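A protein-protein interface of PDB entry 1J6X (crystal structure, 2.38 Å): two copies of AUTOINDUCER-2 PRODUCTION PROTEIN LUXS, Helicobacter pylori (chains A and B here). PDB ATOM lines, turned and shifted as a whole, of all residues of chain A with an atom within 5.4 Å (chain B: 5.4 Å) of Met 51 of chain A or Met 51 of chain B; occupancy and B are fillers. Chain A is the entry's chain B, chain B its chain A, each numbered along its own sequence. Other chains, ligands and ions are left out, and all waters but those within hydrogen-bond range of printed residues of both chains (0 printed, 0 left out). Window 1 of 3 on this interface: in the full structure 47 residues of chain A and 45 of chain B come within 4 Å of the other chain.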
ATOM      1  N   MET A  49      12.179 -21.904 -28.723  1.00  0.00           N
ATOM      2  CA  MET A  49      12.586 -23.022 -29.580  1.00  0.00           C
ATOM      3  C   MET A  49      13.602 -23.891 -28.848  1.00  0.00           C
ATOM      4  O   MET A  49      14.532 -23.345 -28.252  1.00  0.00           O
ATOM      5  CB  MET A  49      13.256 -22.490 -30.862  1.00  0.00           C
ATOM      6  CG  MET A  49      12.382 -21.603 -31.737  1.00  0.00           C
ATOM      7  SD  MET A  49      13.333 -20.840 -33.266  1.00  0.00           S
ATOM      8  CE  MET A  49      14.016 -19.232 -32.430  1.00  0.00           C
ATOM      9  N   ASP A  50      13.459 -25.218 -28.871  1.00  0.00           N
ATOM     10  CA  ASP A  50      14.478 -26.031 -28.207  1.00  0.00           C
ATOM     11  C   ASP A  50      15.716 -25.911 -29.079  1.00  0.00           C
ATOM     12  O   ASP A  50      15.605 -25.773 -30.289  1.00  0.00           O
ATOM     13  CB  ASP A  50      14.068 -27.516 -28.053  1.00  0.00           C
ATOM     14  CG  ASP A  50      13.246 -28.033 -29.214  1.00  0.00           C
ATOM     15  OD1 ASP A  50      12.000 -27.988 -29.093  1.00  0.00           O
ATOM     16  OD2 ASP A  50      13.823 -28.468 -30.241  1.00  0.00           O
ATOM     17  N   MET A  51      16.890 -25.961 -28.463  1.00  0.00           N
ATOM     18  CA  MET A  51      18.141 -25.811 -29.200  1.00  0.00           C
ATOM     19  C   MET A  51      18.390 -26.681 -30.425  1.00  0.00           C
ATOM     20  O   MET A  51      18.957 -26.202 -31.411  1.00  0.00           O
ATOM     21  CB  MET A  51      19.324 -25.918 -28.254  1.00  0.00           C
ATOM     22  CG  MET A  51      19.431 -24.713 -27.328  1.00  0.00           C
ATOM     23  SD  MET A  51      19.340 -22.973 -28.277  1.00  0.00           S
ATOM     24  CE  MET A  51      21.029 -23.071 -29.223  1.00  0.00           C
ATOM     25  N   PRO A  52      18.009 -27.972 -30.385  1.00  0.00           N
ATOM     26  CA  PRO A  52      18.256 -28.776 -31.592  1.00  0.00           C
ATOM     27  C   PRO A  52      17.491 -28.266 -32.820  1.00  0.00           C
ATOM     28  O   PRO A  52      18.047 -28.200 -33.919  1.00  0.00           O
ATOM     29  CB  PRO A  52      17.831 -30.175 -31.159  1.00  0.00           C
ATOM     30  CG  PRO A  52      18.338 -30.205 -29.722  1.00  0.00           C
ATOM     31  CD  PRO A  52      17.845 -28.846 -29.205  1.00  0.00           C
ATOM     32  N   SER A  53      16.224 -27.893 -32.640  1.00  0.00           N
ATOM     33  CA  SER A  53      15.430 -27.383 -33.763  1.00  0.00           C
ATOM     34  C   SER A  53      15.923 -25.988 -34.164  1.00  0.00           C
ATOM     35  O   SER A  53      15.990 -25.667 -35.350  1.00  0.00           O
ATOM     36  CB  SER A  53      13.941 -27.306 -33.400  1.00  0.00           C
ATOM     37  OG  SER A  53      13.441 -28.551 -32.948  1.00  0.00           O
ATOM     38  N   LEU A  54      16.258 -25.167 -33.169  1.00  0.00           N
ATOM     39  CA  LEU A  54      16.758 -23.817 -33.420  1.00  0.00           C
ATOM     40  C   LEU A  54      18.063 -23.898 -34.210  1.00  0.00           C
ATOM     41  O   LEU A  54      18.255 -23.189 -35.205  1.00  0.00           O
ATOM     42  CB  LEU A  54      16.991 -23.072 -32.089  1.00  0.00           C
ATOM     43  CG  LEU A  54      17.662 -21.693 -32.189  1.00  0.00           C
ATOM     44  CD1 LEU A  54      17.349 -20.888 -30.947  1.00  0.00           C
ATOM     45  CD2 LEU A  54      19.176 -21.849 -32.374  1.00  0.00           C
ATOM     46  N   HIS A  55      18.951 -24.772 -33.749  1.00  0.00           N
ATOM     47  CA  HIS A  55      20.245 -24.990 -34.375  1.00  0.00           C
ATOM     48  C   HIS A  55      20.131 -25.457 -35.823  1.00  0.00           C
ATOM     49  O   HIS A  55      20.895 -25.027 -36.684  1.00  0.00           O
ATOM     50  CB  HIS A  55      21.031 -26.031 -33.590  1.00  0.00           C
ATOM     51  CG  HIS A  55      22.429 -26.211 -34.079  1.00  0.00           C
ATOM     52  ND1 HIS A  55      23.198 -27.306 -33.753  1.00  0.00           N
ATOM     53  CD2 HIS A  55      23.202 -25.428 -34.869  1.00  0.00           C
ATOM     54  CE1 HIS A  55      24.384 -27.189 -34.323  1.00  0.00           C
ATOM     55  NE2 HIS A  55      24.411 -26.059 -35.006  1.00  0.00           N
ATOM     56  N   SER A  56      19.181 -26.341 -36.100  1.00  0.00           N
ATOM     57  CA  SER A  56      19.027 -26.836 -37.454  1.00  0.00           C
ATOM     58  C   SER A  56      18.354 -25.834 -38.381  1.00  0.00           C
ATOM     59  O   SER A  56      18.700 -25.733 -39.559  1.00  0.00           O
ATOM     60  CB  SER A  56      18.252 -28.156 -37.443  1.00  0.00           C
ATOM     61  OG  SER A  56      19.060 -29.185 -36.889  1.00  0.00           O
ATOM     62  N   MET A  78      18.847 -15.822 -31.771  1.00  0.00           N
ATOM     63  CA  MET A  78      18.905 -14.968 -30.601  1.00  0.00           C
ATOM     64  C   MET A  78      19.203 -15.862 -29.406  1.00  0.00           C
ATOM     65  O   MET A  78      18.800 -17.033 -29.378  1.00  0.00           O
ATOM     66  CB  MET A  78      17.565 -14.278 -30.403  1.00  0.00           C
ATOM     67  CG  MET A  78      17.249 -13.241 -31.464  1.00  0.00           C
ATOM     68  SD  MET A  78      15.442 -12.605 -31.285  1.00  0.00           S
ATOM     69  CE  MET A  78      15.350 -11.532 -32.888  1.00  0.00           C
ATOM     70  N   GLY A  79      19.901 -15.323 -28.419  1.00  0.00           N
ATOM     71  CA  GLY A  79      20.208 -16.120 -27.247  1.00  0.00           C
ATOM     72  C   GLY A  79      18.943 -16.468 -26.477  1.00  0.00           C
ATOM     73  O   GLY A  79      18.897 -17.455 -25.742  1.00  0.00           O
ATOM     74  N   GLN A  81      16.384 -17.633 -27.635  1.00  0.00           N
ATOM     75  CA  GLN A  81      15.728 -18.742 -28.320  1.00  0.00           C
ATOM     76  C   GLN A  81      14.331 -18.454 -28.870  1.00  0.00           C
ATOM     77  O   GLN A  81      13.576 -19.393 -29.154  1.00  0.00           O
ATOM     78  CB  GLN A  81      15.656 -19.960 -27.387  1.00  0.00           C
ATOM     79  CG  GLN A  81      16.991 -20.358 -26.797  1.00  0.00           C
ATOM     80  CD  GLN A  81      16.952 -21.630 -25.953  1.00  0.00           C
ATOM     81  OE1 GLN A  81      17.616 -21.715 -24.925  1.00  0.00           O
ATOM     82  NE2 GLN A  81      16.208 -22.628 -26.402  1.00  0.00           N
ATOM     83  N   ASN A 127      23.871 -32.182 -31.988  1.00  0.00           N
ATOM     84  CA  ASN A 127      22.670 -31.427 -31.610  1.00  0.00           C
ATOM     85  C   ASN A 127      21.847 -30.880 -32.780  1.00  0.00           C
ATOM     86  O   ASN A 127      21.740 -29.669 -32.965  1.00  0.00           O
ATOM     87  CB  ASN A 127      23.073 -30.280 -30.682  1.00  0.00           C
ATOM     88  CG  ASN A 127      22.128 -30.123 -29.515  1.00  0.00           C
ATOM     89  OD1 ASN A 127      21.674 -31.111 -28.946  1.00  0.00           O
ATOM     90  ND2 ASN A 127      21.839 -28.879 -29.135  1.00  0.00           N
ATOM     91  N   MET B  49      28.792 -24.198 -24.365  1.00  0.00           N
ATOM     92  CA  MET B  49      28.294 -23.320 -23.306  1.00  0.00           C
ATOM     93  C   MET B  49      26.830 -23.632 -23.023  1.00  0.00           C
ATOM     94  O   MET B  49      26.052 -23.892 -23.948  1.00  0.00           O
ATOM     95  CB  MET B  49      28.370 -21.847 -23.726  1.00  0.00           C
ATOM     96  CG  MET B  49      29.740 -21.283 -24.032  1.00  0.00           C
ATOM     97  SD  MET B  49      29.582 -19.463 -24.759  1.00  0.00           S
ATOM     98  CE  MET B  49      29.549 -19.911 -26.622  1.00  0.00           C
ATOM     99  N   ASP B  50      26.453 -23.593 -21.750  1.00  0.00           N
ATOM    100  CA  ASP B  50      25.061 -23.822 -21.351  1.00  0.00           C
ATOM    101  C   ASP B  50      24.310 -22.533 -21.699  1.00  0.00           C
ATOM    102  O   ASP B  50      24.823 -21.434 -21.482  1.00  0.00           O
ATOM    103  CB  ASP B  50      24.967 -24.052 -19.846  1.00  0.00           C
ATOM    104  CG  ASP B  50      25.585 -22.920 -19.062  1.00  0.00           C
ATOM    105  OD1 ASP B  50      24.885 -22.352 -18.195  1.00  0.00           O
ATOM    106  OD2 ASP B  50      26.774 -22.593 -19.323  1.00  0.00           O
ATOM    107  N   MET B  51      23.097 -22.678 -22.206  1.00  0.00           N
ATOM    108  CA  MET B  51      22.288 -21.547 -22.617  1.00  0.00           C
ATOM    109  C   MET B  51      22.118 -20.371 -21.669  1.00  0.00           C
ATOM    110  O   MET B  51      22.216 -19.225 -22.098  1.00  0.00           O
ATOM    111  CB  MET B  51      20.921 -22.033 -23.073  1.00  0.00           C
ATOM    112  CG  MET B  51      20.985 -22.767 -24.410  1.00  0.00           C
ATOM    113  SD  MET B  51      22.006 -21.790 -25.770  1.00  0.00           S
ATOM    114  CE  MET B  51      20.946 -20.176 -25.860  1.00  0.00           C
ATOM    115  N   PRO B  52      21.856 -20.622 -20.376  1.00  0.00           N
ATOM    116  CA  PRO B  52      21.702 -19.451 -19.504  1.00  0.00           C
ATOM    117  C   PRO B  52      22.969 -18.605 -19.428  1.00  0.00           C
ATOM    118  O   PRO B  52      22.902 -17.381 -19.427  1.00  0.00           O
ATOM    119  CB  PRO B  52      21.318 -20.065 -18.155  1.00  0.00           C
ATOM    120  CG  PRO B  52      20.583 -21.320 -18.556  1.00  0.00           C
ATOM    121  CD  PRO B  52      21.469 -21.857 -19.672  1.00  0.00           C
ATOM    122  N   SER B  53      24.126 -19.246 -19.375  1.00  0.00           N
ATOM    123  CA  SER B  53      25.375 -18.491 -19.301  1.00  0.00           C
ATOM    124  C   SER B  53      25.651 -17.786 -20.631  1.00  0.00           C
ATOM    125  O   SER B  53      26.139 -16.654 -20.668  1.00  0.00           O
ATOM    126  CB  SER B  53      26.546 -19.414 -18.953  1.00  0.00           C
ATOM    127  OG  SER B  53      26.418 -19.956 -17.646  1.00  0.00           O
ATOM    128  N   LEU B  54      25.327 -18.472 -21.717  1.00  0.00           N
ATOM    129  CA  LEU B  54      25.520 -17.963 -23.066  1.00  0.00           C
ATOM    130  C   LEU B  54      24.584 -16.771 -23.295  1.00  0.00           C
ATOM    131  O   LEU B  54      24.995 -15.754 -23.837  1.00  0.00           O
ATOM    132  CB  LEU B  54      25.235 -19.090 -24.066  1.00  0.00           C
ATOM    133  CG  LEU B  54      25.254 -18.876 -25.580  1.00  0.00           C
ATOM    134  CD1 LEU B  54      25.443 -20.218 -26.284  1.00  0.00           C
ATOM    135  CD2 LEU B  54      23.940 -18.229 -26.035  1.00  0.00           C
ATOM    136  N   HIS B  55      23.335 -16.906 -22.858  1.00  0.00           N
ATOM    137  CA  HIS B  55      22.354 -15.858 -23.004  1.00  0.00           C
ATOM    138  C   HIS B  55      22.784 -14.598 -22.261  1.00  0.00           C
ATOM    139  O   HIS B  55      22.680 -13.483 -22.791  1.00  0.00           O
ATOM    140  CB  HIS B  55      20.997 -16.317 -22.474  1.00  0.00           C
ATOM    141  CG  HIS B  55      19.882 -15.363 -22.782  1.00  0.00           C
ATOM    142  ND1 HIS B  55      18.616 -15.488 -22.246  1.00  0.00           N
ATOM    143  CD2 HIS B  55      19.845 -14.269 -23.580  1.00  0.00           C
ATOM    144  CE1 HIS B  55      17.849 -14.514 -22.698  1.00  0.00           C
ATOM    145  NE2 HIS B  55      18.571 -13.761 -23.508  1.00  0.00           N
ATOM    146  N   SER B  56      23.260 -14.784 -21.032  1.00  0.00           N
ATOM    147  CA  SER B  56      23.711 -13.670 -20.210  1.00  0.00           C
ATOM    148  C   SER B  56      24.953 -13.017 -20.794  1.00  0.00           C
ATOM    149  O   SER B  56      25.100 -11.794 -20.717  1.00  0.00           O
ATOM    150  CB  SER B  56      23.988 -14.132 -18.786  1.00  0.00           C
ATOM    151  OG  SER B  56      22.779 -14.155 -18.052  1.00  0.00           O
ATOM    152  N   MET B  78      26.288 -18.377 -31.513  1.00  0.00           N
ATOM    153  CA  MET B  78      26.174 -19.370 -32.586  1.00  0.00           C
ATOM    154  C   MET B  78      25.196 -20.474 -32.147  1.00  0.00           C
ATOM    155  O   MET B  78      25.084 -20.783 -30.958  1.00  0.00           O
ATOM    156  CB  MET B  78      27.523 -20.004 -32.881  1.00  0.00           C
ATOM    157  CG  MET B  78      28.506 -19.112 -33.575  1.00  0.00           C
ATOM    158  SD  MET B  78      30.278 -19.898 -33.464  1.00  0.00           S
ATOM    159  CE  MET B  78      31.362 -18.310 -33.717  1.00  0.00           C
ATOM    160  N   GLY B  79      24.501 -21.072 -33.112  1.00  0.00           N
ATOM    161  CA  GLY B  79      23.550 -22.119 -32.790  1.00  0.00           C
ATOM    162  C   GLY B  79      24.188 -23.348 -32.176  1.00  0.00           C
ATOM    163  O   GLY B  79      23.513 -24.107 -31.504  1.00  0.00           O
ATOM    164  N   GLN B  81      26.502 -23.303 -29.883  1.00  0.00           N
ATOM    165  CA  GLN B  81      26.885 -23.032 -28.500  1.00  0.00           C
ATOM    166  C   GLN B  81      28.373 -23.082 -28.160  1.00  0.00           C
ATOM    167  O   GLN B  81      28.722 -23.358 -27.016  1.00  0.00           O
ATOM    168  CB  GLN B  81      26.129 -24.001 -27.571  1.00  0.00           C
ATOM    169  CG  GLN B  81      24.681 -23.606 -27.319  1.00  0.00           C
ATOM    170  CD  GLN B  81      23.874 -24.704 -26.647  1.00  0.00           C
ATOM    171  OE1 GLN B  81      23.222 -25.491 -27.318  1.00  0.00           O
ATOM    172  NE2 GLN B  81      23.927 -24.763 -25.314  1.00  0.00           N
ATOM    173  N   ASN B 127      15.783 -17.054 -18.161  1.00  0.00           N
ATOM    174  CA  ASN B 127      16.958 -17.845 -18.536  1.00  0.00           C
ATOM    175  C   ASN B 127      18.269 -17.070 -18.550  1.00  0.00           C
ATOM    176  O   ASN B 127      18.829 -16.794 -19.605  1.00  0.00           O
ATOM    177  CB  ASN B 127      16.721 -18.490 -19.903  1.00  0.00           C
ATOM    178  CG  ASN B 127      17.357 -19.860 -20.012  1.00  0.00           C
ATOM    179  OD1 ASN B 127      17.242 -20.667 -19.098  1.00  0.00           O
ATOM    180  ND2 ASN B 127      18.018 -20.135 -21.134  1.00  0.00           N
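Met 51 of chain B touches just these residues of chain A: Met 51, Gly 79 and Gln 81. Of the printed residues of chain B, Gln 81 of chain A touches Met 51 (3.6 Å). Of the printed residues of chain A, Gln 81 of chain B touches Met 51. Leu 54 of chain B touches none of the printed residues of chain A. Ser 56 of chain B touches none of the printed residues of chain A. The nearest residue of chain B that does not touch Met 51 of chain A is Met 78 of chain B (5.0 Å). The nearest residue of chain A that does not touch Met 51 of chain B is Met 78 of chain A (5.2 Å).
The backbone carbonyl oxygen (O) of Met 49 of chain B sits at hydrogen-bond distance from the side-chain amide nitrogen (NE2) of Gln 81 of chain B. SD of Met 51 of chain B sits at hydrogen-bond distance from NE2 of Gln 81 of chain B, at 3.6 Å. The backbone carbonyl oxygen of Asn 127 of chain B lies within hydrogen-bond range of a ring nitrogen (ND1) of His 55 of chain B, 3.0 Å away. NE2 of Gln 81 of chain A lies within hydrogen-bond range of O of Met 49 of chain A, at 2.6 Å. SD of Met 51 of chain A lies close to NE2 of Gln 81 of chain A, 3.7 Å away. A ring nitrogen (ND1) of His 55 of chain A sits at hydrogen-bond distance from the backbone carbonyl oxygen (O) of Asn 127 of chain A, at 2.9 Å.
Of the 12 printed residues of chain B, 4 touch a printed residue of chain A. Hydrophobic or aromatic side chains of chain B within 4 Å of the printed part of chain A: Met 51 and His 55. Of the 12 printed residues of chain A, 4 touch a printed residue of chain B. Hydrophobic or aromatic side chains of chain A that line the printed part of chain B: Met 51 and His 55. Among the printed residues, 7 pairs touch across the chains.
Met 51 of chain B touches its own counterpart, Met 51 of chain A. Met 51 of chain A touches Gly 79 of chain B, and with the chains exchanged Gly 79 of chain A touches Met 51 of chain B. Met 51 of chain A touches Gln 81 of chain B, and with the chains exchanged Gln 81 of chain A touches Met 51 of chain B. His 55 of chain A touches Gly 79 of chain B, and with the chains exchanged Gly 79 of chain A touches His 55 of chain B.
Among the printed residues, pairs that only touch across the chains: Gly 79 of chain A with Met 51 of chain B (3.4 Å), His 55 of chain A with Gly 79 of chain B (3.5 Å), Met 51 of chain A with Gly 79 of chain B (3.5 Å), Gln 81 of chain A with Met 51 of chain B (3.6 Å), Gly 79 of chain A with His 55 of chain B (3.7 Å), Met 51 of chain A with Gln 81 of chain B (3.8 Å) and Met 51 of chain A with Met 51 of chain B (3.8 Å).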
